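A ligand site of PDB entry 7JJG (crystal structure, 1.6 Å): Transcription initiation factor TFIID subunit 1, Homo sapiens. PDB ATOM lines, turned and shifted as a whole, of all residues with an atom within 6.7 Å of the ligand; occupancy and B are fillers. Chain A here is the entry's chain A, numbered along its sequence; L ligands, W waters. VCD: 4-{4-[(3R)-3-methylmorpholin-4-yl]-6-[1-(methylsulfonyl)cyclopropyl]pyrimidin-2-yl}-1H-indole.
The backbone NH (N) of Asn 35 lies within hydrogen-bond range of an oxygen (O26) of the ligand, 2.9 Å away. O10 of the ligand is in hydrogen-bond range of ND2 of Asn 85.
ND2 of Asn 85 sits at hydrogen-bond distance from OG of Ser 81 (3.1 Å).
O27 of the ligand lies close to O of Pro 33. Merely in contact with the ligand: Trp 28 (3.5 Å), Pro 29 (3.4 Å), Phe 30 (3.8 Å), His 32 (3.1 Å), Val 34 (3.7 Å), Phe 38 (3.6 Å), Val 39 (3.8 Å), Tyr 84 (3.9 Å) and Tyr 91 (3.6 Å). 12 residues have an atom within 4 Å of the ligand: Trp 28, Pro 29, Phe 30, His 32, Pro 33, Val 34, Asn 35, Phe 38, Val 39, Tyr 84, Asn 85 and Tyr 91.
Water W2 bridges O of Pro 33 (2.7 Å) and O27 of the ligand (3.1 Å). Water W1 bridges the side-chain amide nitrogen of Asn 35 (3.1 Å) and an oxygen (O27) of the ligand (3.5 Å).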
ATOM      1  N   TRP A  28     -15.170  21.534  20.187  1.00  0.00           N
ATOM      2  CA  TRP A  28     -14.872  21.897  18.799  1.00  0.00           C
ATOM      3  C   TRP A  28     -13.397  21.706  18.413  1.00  0.00           C
ATOM      4  O   TRP A  28     -13.128  21.338  17.248  1.00  0.00           O
ATOM      5  CB  TRP A  28     -15.325  23.369  18.476  1.00  0.00           C
ATOM      6  CG  TRP A  28     -14.601  24.363  19.300  1.00  0.00           C
ATOM      7  CD1 TRP A  28     -15.010  24.895  20.484  1.00  0.00           C
ATOM      8  CD2 TRP A  28     -13.302  24.921  19.036  1.00  0.00           C
ATOM      9  NE1 TRP A  28     -14.047  25.720  20.985  1.00  0.00           N
ATOM     10  CE2 TRP A  28     -12.995  25.767  20.112  1.00  0.00           C
ATOM     11  CE3 TRP A  28     -12.378  24.784  17.995  1.00  0.00           C
ATOM     12  CZ2 TRP A  28     -11.781  26.448  20.196  1.00  0.00           C
ATOM     13  CZ3 TRP A  28     -11.186  25.485  18.075  1.00  0.00           C
ATOM     14  CH2 TRP A  28     -10.893  26.292  19.174  1.00  0.00           C
ATOM     15  N   PRO A  29     -12.406  21.893  19.283  1.00  0.00           N
ATOM     16  CA  PRO A  29     -11.012  21.761  18.790  1.00  0.00           C
ATOM     17  C   PRO A  29     -10.678  20.383  18.286  1.00  0.00           C
ATOM     18  O   PRO A  29      -9.690  20.221  17.544  1.00  0.00           O
ATOM     19  CB  PRO A  29     -10.154  22.104  20.010  1.00  0.00           C
ATOM     20  CG  PRO A  29     -11.061  22.837  20.947  1.00  0.00           C
ATOM     21  CD  PRO A  29     -12.412  22.253  20.726  1.00  0.00           C
ATOM     22  N   PHE A  30     -11.466  19.380  18.679  1.00  0.00           N
ATOM     23  CA  PHE A  30     -11.178  17.965  18.427  1.00  0.00           C
ATOM     24  C   PHE A  30     -12.142  17.335  17.451  1.00  0.00           C
ATOM     25  O   PHE A  30     -12.066  16.121  17.184  1.00  0.00           O
ATOM     26  CB  PHE A  30     -11.169  17.246  19.785  1.00  0.00           C
ATOM     27  CG  PHE A  30     -10.290  17.907  20.783  1.00  0.00           C
ATOM     28  CD1 PHE A  30      -8.918  17.892  20.640  1.00  0.00           C
ATOM     29  CD2 PHE A  30     -10.829  18.617  21.848  1.00  0.00           C
ATOM     30  CE1 PHE A  30      -8.091  18.540  21.535  1.00  0.00           C
ATOM     31  CE2 PHE A  30     -10.013  19.258  22.745  1.00  0.00           C
ATOM     32  CZ  PHE A  30      -8.658  19.206  22.608  1.00  0.00           C
ATOM     33  N   HIS A  31     -13.041  18.124  16.857  1.00  0.00           N
ATOM     34  CA  HIS A  31     -14.041  17.538  15.990  1.00  0.00           C
ATOM     35  C   HIS A  31     -13.547  17.226  14.589  1.00  0.00           C
ATOM     36  O   HIS A  31     -14.186  16.433  13.898  1.00  0.00           O
ATOM     37  CB  HIS A  31     -15.260  18.465  15.846  1.00  0.00           C
ATOM     38  CG  HIS A  31     -16.181  18.466  17.032  1.00  0.00           C
ATOM     39  ND1 HIS A  31     -17.491  18.881  16.922  1.00  0.00           N
ATOM     40  CD2 HIS A  31     -15.987  18.151  18.331  1.00  0.00           C
ATOM     41  CE1 HIS A  31     -18.084  18.773  18.106  1.00  0.00           C
ATOM     42  NE2 HIS A  31     -17.186  18.365  18.984  1.00  0.00           N
ATOM     43  N   HIS A  32     -12.472  17.860  14.146  1.00  0.00           N
ATOM     44  CA  HIS A  32     -11.982  17.785  12.789  1.00  0.00           C
ATOM     45  C   HIS A  32     -10.459  17.819  12.831  1.00  0.00           C
ATOM     46  O   HIS A  32      -9.895  18.306  13.817  1.00  0.00           O
ATOM     47  CB  HIS A  32     -12.471  18.979  11.945  1.00  0.00           C
ATOM     48  CG  HIS A  32     -13.957  19.058  11.859  1.00  0.00           C
ATOM     49  ND1 HIS A  32     -14.692  18.176  11.109  1.00  0.00           N
ATOM     50  CD2 HIS A  32     -14.837  19.887  12.455  1.00  0.00           C
ATOM     51  CE1 HIS A  32     -15.977  18.457  11.247  1.00  0.00           C
ATOM     52  NE2 HIS A  32     -16.096  19.495  12.059  1.00  0.00           N
ATOM     53  N   PRO A  33      -9.799  17.367  11.776  1.00  0.00           N
ATOM     54  CA  PRO A  33      -8.351  17.598  11.683  1.00  0.00           C
ATOM     55  C   PRO A  33      -8.035  19.089  11.693  1.00  0.00           C
ATOM     56  O   PRO A  33      -8.773  19.896  11.111  1.00  0.00           O
ATOM     57  CB  PRO A  33      -7.934  16.955  10.355  1.00  0.00           C
ATOM     58  CG  PRO A  33      -9.118  16.275   9.824  1.00  0.00           C
ATOM     59  CD  PRO A  33     -10.332  16.714  10.563  1.00  0.00           C
ATOM     60  N   VAL A  34      -6.934  19.432  12.345  1.00  0.00           N
ATOM     61  CA  VAL A  34      -6.436  20.805  12.313  1.00  0.00           C
ATOM     62  C   VAL A  34      -6.110  21.195  10.885  1.00  0.00           C
ATOM     63  O   VAL A  34      -5.452  20.446  10.140  1.00  0.00           O
ATOM     64  CB  VAL A  34      -5.211  20.938  13.237  1.00  0.00           C
ATOM     65  CG1 VAL A  34      -4.623  22.323  13.125  1.00  0.00           C
ATOM     66  CG2 VAL A  34      -5.609  20.631  14.665  1.00  0.00           C
ATOM     67  N   ASN A  35      -6.575  22.370  10.481  1.00  0.00           N
ATOM     68  CA  ASN A  35      -6.279  22.923   9.173  1.00  0.00           C
ATOM     69  C   ASN A  35      -4.881  23.517   9.194  1.00  0.00           C
ATOM     70  O   ASN A  35      -4.605  24.429   9.980  1.00  0.00           O
ATOM     71  CB  ASN A  35      -7.344  23.962   8.844  1.00  0.00           C
ATOM     72  CG  ASN A  35      -7.200  24.565   7.487  1.00  0.00           C
ATOM     73  OD1 ASN A  35      -6.113  24.589   6.901  1.00  0.00           O
ATOM     74  ND2 ASN A  35      -8.321  25.070   6.949  1.00  0.00           N
ATOM     75  N   LYS A  36      -3.995  22.979   8.347  1.00  0.00           N
ATOM     76  CA  LYS A  36      -2.598  23.404   8.357  1.00  0.00           C
ATOM     77  C   LYS A  36      -2.446  24.873   7.997  1.00  0.00           C
ATOM     78  O   LYS A  36      -1.461  25.510   8.396  1.00  0.00           O
ATOM     79  CB  LYS A  36      -1.810  22.529   7.373  1.00  0.00           C
ATOM     80  CG  LYS A  36      -0.328  22.840   7.280  1.00  0.00           C
ATOM     81  CD  LYS A  36       0.336  21.963   6.211  1.00  0.00           C
ATOM     82  CE  LYS A  36       0.394  20.512   6.668  1.00  0.00           C
ATOM     83  NZ  LYS A  36       1.495  19.725   6.020  1.00  0.00           N
ATOM     84  N   PHE A  38      -4.492  27.158   9.032  1.00  0.00           N
ATOM     85  CA  PHE A  38      -4.844  27.880  10.240  1.00  0.00           C
ATOM     86  C   PHE A  38      -3.803  27.738  11.339  1.00  0.00           C
ATOM     87  O   PHE A  38      -3.590  28.678  12.113  1.00  0.00           O
ATOM     88  CB  PHE A  38      -6.189  27.382  10.782  1.00  0.00           C
ATOM     89  CG  PHE A  38      -7.371  27.739   9.952  1.00  0.00           C
ATOM     90  CD1 PHE A  38      -7.315  28.757   9.008  1.00  0.00           C
ATOM     91  CD2 PHE A  38      -8.570  27.073  10.128  1.00  0.00           C
ATOM     92  CE1 PHE A  38      -8.423  29.072   8.252  1.00  0.00           C
ATOM     93  CE2 PHE A  38      -9.672  27.390   9.365  1.00  0.00           C
ATOM     94  CZ  PHE A  38      -9.600  28.399   8.434  1.00  0.00           C
ATOM     95  N   VAL A  39      -3.156  26.575  11.435  1.00  0.00           N
ATOM     96  CA  VAL A  39      -2.184  26.321  12.496  1.00  0.00           C
ATOM     97  C   VAL A  39      -0.953  25.724  11.844  1.00  0.00           C
ATOM     98  O   VAL A  39      -0.727  24.506  11.917  1.00  0.00           O
ATOM     99  CB  VAL A  39      -2.760  25.412  13.582  1.00  0.00           C
ATOM    100  CG1 VAL A  39      -1.849  25.383  14.769  1.00  0.00           C
ATOM    101  CG2 VAL A  39      -4.151  25.918  13.981  1.00  0.00           C
ATOM    102  N   TYR A  42       1.268  23.022  13.541  1.00  0.00           N
ATOM    103  CA  TYR A  42       0.658  21.886  14.224  1.00  0.00           C
ATOM    104  C   TYR A  42       1.312  20.588  13.805  1.00  0.00           C
ATOM    105  O   TYR A  42       1.632  19.724  14.637  1.00  0.00           O
ATOM    106  CB  TYR A  42      -0.851  21.827  13.962  1.00  0.00           C
ATOM    107  CG  TYR A  42      -1.527  20.788  14.843  1.00  0.00           C
ATOM    108  CD1 TYR A  42      -1.769  21.052  16.181  1.00  0.00           C
ATOM    109  CD2 TYR A  42      -1.871  19.543  14.342  1.00  0.00           C
ATOM    110  CE1 TYR A  42      -2.339  20.118  16.984  1.00  0.00           C
ATOM    111  CE2 TYR A  42      -2.466  18.585  15.159  1.00  0.00           C
ATOM    112  CZ  TYR A  42      -2.701  18.886  16.482  1.00  0.00           C
ATOM    113  OH  TYR A  42      -3.296  17.943  17.301  1.00  0.00           O
ATOM    114  N   ASP A  51      -8.445  12.923  15.439  1.00  0.00           N
ATOM    115  CA  ASP A  51      -9.581  13.783  15.740  1.00  0.00           C
ATOM    116  C   ASP A  51     -10.842  12.952  15.591  1.00  0.00           C
ATOM    117  O   ASP A  51     -10.801  11.830  15.062  1.00  0.00           O
ATOM    118  CB  ASP A  51      -9.617  14.981  14.805  1.00  0.00           C
ATOM    119  CG  ASP A  51      -9.834  14.553  13.394  1.00  0.00           C
ATOM    120  OD1 ASP A  51      -8.826  14.258  12.705  1.00  0.00           O
ATOM    121  OD2 ASP A  51     -11.010  14.473  12.982  1.00  0.00           O
ATOM    122  N   ASN A  80      -2.055  14.051  22.052  1.00  0.00           N
ATOM    123  CA  ASN A  80      -1.615  15.143  21.194  1.00  0.00           C
ATOM    124  C   ASN A  80      -1.943  16.488  21.806  1.00  0.00           C
ATOM    125  O   ASN A  80      -1.239  17.476  21.526  1.00  0.00           O
ATOM    126  CB  ASN A  80      -2.249  15.017  19.815  1.00  0.00           C
ATOM    127  CG  ASN A  80      -1.675  13.888  19.008  1.00  0.00           C
ATOM    128  OD1 ASN A  80      -0.575  13.390  19.283  1.00  0.00           O
ATOM    129  ND2 ASN A  80      -2.416  13.477  17.981  1.00  0.00           N
ATOM    130  N   SER A  81      -3.007  16.583  22.607  1.00  0.00           N
ATOM    131  CA  SER A  81      -3.272  17.859  23.280  1.00  0.00           C
ATOM    132  C   SER A  81      -2.259  18.099  24.395  1.00  0.00           C
ATOM    133  O   SER A  81      -1.826  19.229  24.608  1.00  0.00           O
ATOM    134  CB  SER A  81      -4.684  17.897  23.851  1.00  0.00           C
ATOM    135  OG  SER A  81      -4.956  19.174  24.383  1.00  0.00           O
ATOM    136  N   TYR A  84       0.833  19.301  22.401  1.00  0.00           N
ATOM    137  CA  TYR A  84       0.801  20.579  21.712  1.00  0.00           C
ATOM    138  C   TYR A  84       0.454  21.723  22.658  1.00  0.00           C
ATOM    139  O   TYR A  84       1.003  22.830  22.539  1.00  0.00           O
ATOM    140  CB  TYR A  84      -0.210  20.545  20.547  1.00  0.00           C
ATOM    141  CG  TYR A  84      -0.022  21.734  19.638  1.00  0.00           C
ATOM    142  CD1 TYR A  84       1.013  21.766  18.708  1.00  0.00           C
ATOM    143  CD2 TYR A  84      -0.847  22.849  19.726  1.00  0.00           C
ATOM    144  CE1 TYR A  84       1.199  22.852  17.890  1.00  0.00           C
ATOM    145  CE2 TYR A  84      -0.645  23.949  18.912  1.00  0.00           C
ATOM    146  CZ  TYR A  84       0.383  23.944  17.998  1.00  0.00           C
ATOM    147  OH  TYR A  84       0.586  25.030  17.182  1.00  0.00           O
ATOM    148  N   ASN A  85      -0.457  21.494  23.605  1.00  0.00           N
ATOM    149  CA  ASN A  85      -1.031  22.537  24.427  1.00  0.00           C
ATOM    150  C   ASN A  85      -0.510  22.510  25.858  1.00  0.00           C
ATOM    151  O   ASN A  85      -0.567  23.537  26.536  1.00  0.00           O
ATOM    152  CB  ASN A  85      -2.557  22.394  24.463  1.00  0.00           C
ATOM    153  CG  ASN A  85      -3.164  22.531  23.104  1.00  0.00           C
ATOM    154  OD1 ASN A  85      -2.947  23.524  22.424  1.00  0.00           O
ATOM    155  ND2 ASN A  85      -3.906  21.505  22.680  1.00  0.00           N
ATOM    156  N   TYR A  91      -7.485  23.165  26.770  1.00  0.00           N
ATOM    157  CA  TYR A  91      -7.711  22.232  25.672  1.00  0.00           C
ATOM    158  C   TYR A  91      -7.581  20.795  26.156  1.00  0.00           C
ATOM    159  O   TYR A  91      -8.374  19.925  25.790  1.00  0.00           O
ATOM    160  CB  TYR A  91      -6.720  22.462  24.541  1.00  0.00           C
ATOM    161  CG  TYR A  91      -6.979  23.689  23.666  1.00  0.00           C
ATOM    162  CD1 TYR A  91      -8.080  23.756  22.842  1.00  0.00           C
ATOM    163  CD2 TYR A  91      -6.080  24.733  23.651  1.00  0.00           C
ATOM    164  CE1 TYR A  91      -8.298  24.862  22.041  1.00  0.00           C
ATOM    165  CE2 TYR A  91      -6.306  25.852  22.860  1.00  0.00           C
ATOM    166  CZ  TYR A  91      -7.421  25.908  22.061  1.00  0.00           C
ATOM    167  OH  TYR A  91      -7.640  27.014  21.260  1.00  0.00           O
HETATM  168  C11 VCD L   1      -6.256  21.287  19.666  1.00  0.00           C
HETATM  169  C01 VCD L   1      -8.239  23.041  16.192  1.00  0.00           C
HETATM  170  C02 VCD L   1      -8.856  23.672  15.112  1.00  0.00           C
HETATM  171  C04 VCD L   1      -7.832  25.736  15.763  1.00  0.00           C
HETATM  172  C06 VCD L   1      -7.425  23.783  17.076  1.00  0.00           C
HETATM  173  C08 VCD L   1      -5.588  23.950  18.709  1.00  0.00           C
HETATM  174  C09 VCD L   1      -5.296  23.431  20.148  1.00  0.00           C
HETATM  175  C12 VCD L   1      -6.753  21.779  18.282  1.00  0.00           C
HETATM  176  C13 VCD L   1      -4.331  23.795  17.804  1.00  0.00           C
HETATM  177  C14 VCD L   1      -7.575  27.097  15.510  1.00  0.00           C
HETATM  178  C15 VCD L   1      -7.597  27.551  14.157  1.00  0.00           C
HETATM  179  C16 VCD L   1      -7.320  28.892  13.838  1.00  0.00           C
HETATM  180  C17 VCD L   1      -7.000  29.825  14.831  1.00  0.00           C
HETATM  181  C18 VCD L   1      -6.951  29.389  16.156  1.00  0.00           C
HETATM  182  C19 VCD L   1      -7.232  28.060  16.501  1.00  0.00           C
HETATM  183  C20 VCD L   1      -7.100  27.990  17.886  1.00  0.00           C
HETATM  184  C21 VCD L   1      -6.749  29.262  18.329  1.00  0.00           C
HETATM  185  C23 VCD L   1      -9.718  22.926  14.185  1.00  0.00           C
HETATM  186  C25 VCD L   1     -10.712  25.174  12.667  1.00  0.00           C
HETATM  187  C28 VCD L   1      -9.768  21.400  14.195  1.00  0.00           C
HETATM  188  C29 VCD L   1     -10.958  22.213  14.711  1.00  0.00           C
HETATM  189  N03 VCD L   1      -8.607  24.997  14.929  1.00  0.00           N
HETATM  190  N05 VCD L   1      -7.228  25.101  16.803  1.00  0.00           N
HETATM  191  N07 VCD L   1      -6.752  23.237  18.164  1.00  0.00           N
HETATM  192  N22 VCD L   1      -6.675  30.094  17.266  1.00  0.00           N
HETATM  193  O10 VCD L   1      -5.104  22.019  20.108  1.00  0.00           O
HETATM  194  O26 VCD L   1      -8.351  23.963  12.057  1.00  0.00           O
HETATM  195  O27 VCD L   1     -10.581  22.579  11.645  1.00  0.00           O
HETATM  196  S24 VCD L   1      -9.793  23.615  12.505  1.00  0.00           S
HETATM  197  O   HOH W   1     -10.803  23.936   8.448  1.00  0.00           O
HETATM  198  O   HOH W   2     -10.038  21.108   9.025  1.00  0.00           O
HETATM  199  O   HOH W   3      -5.786  28.953  21.559  1.00  0.00           O
HETATM  200  O   HOH W   4     -13.534  23.207  10.646  1.00  0.00           O
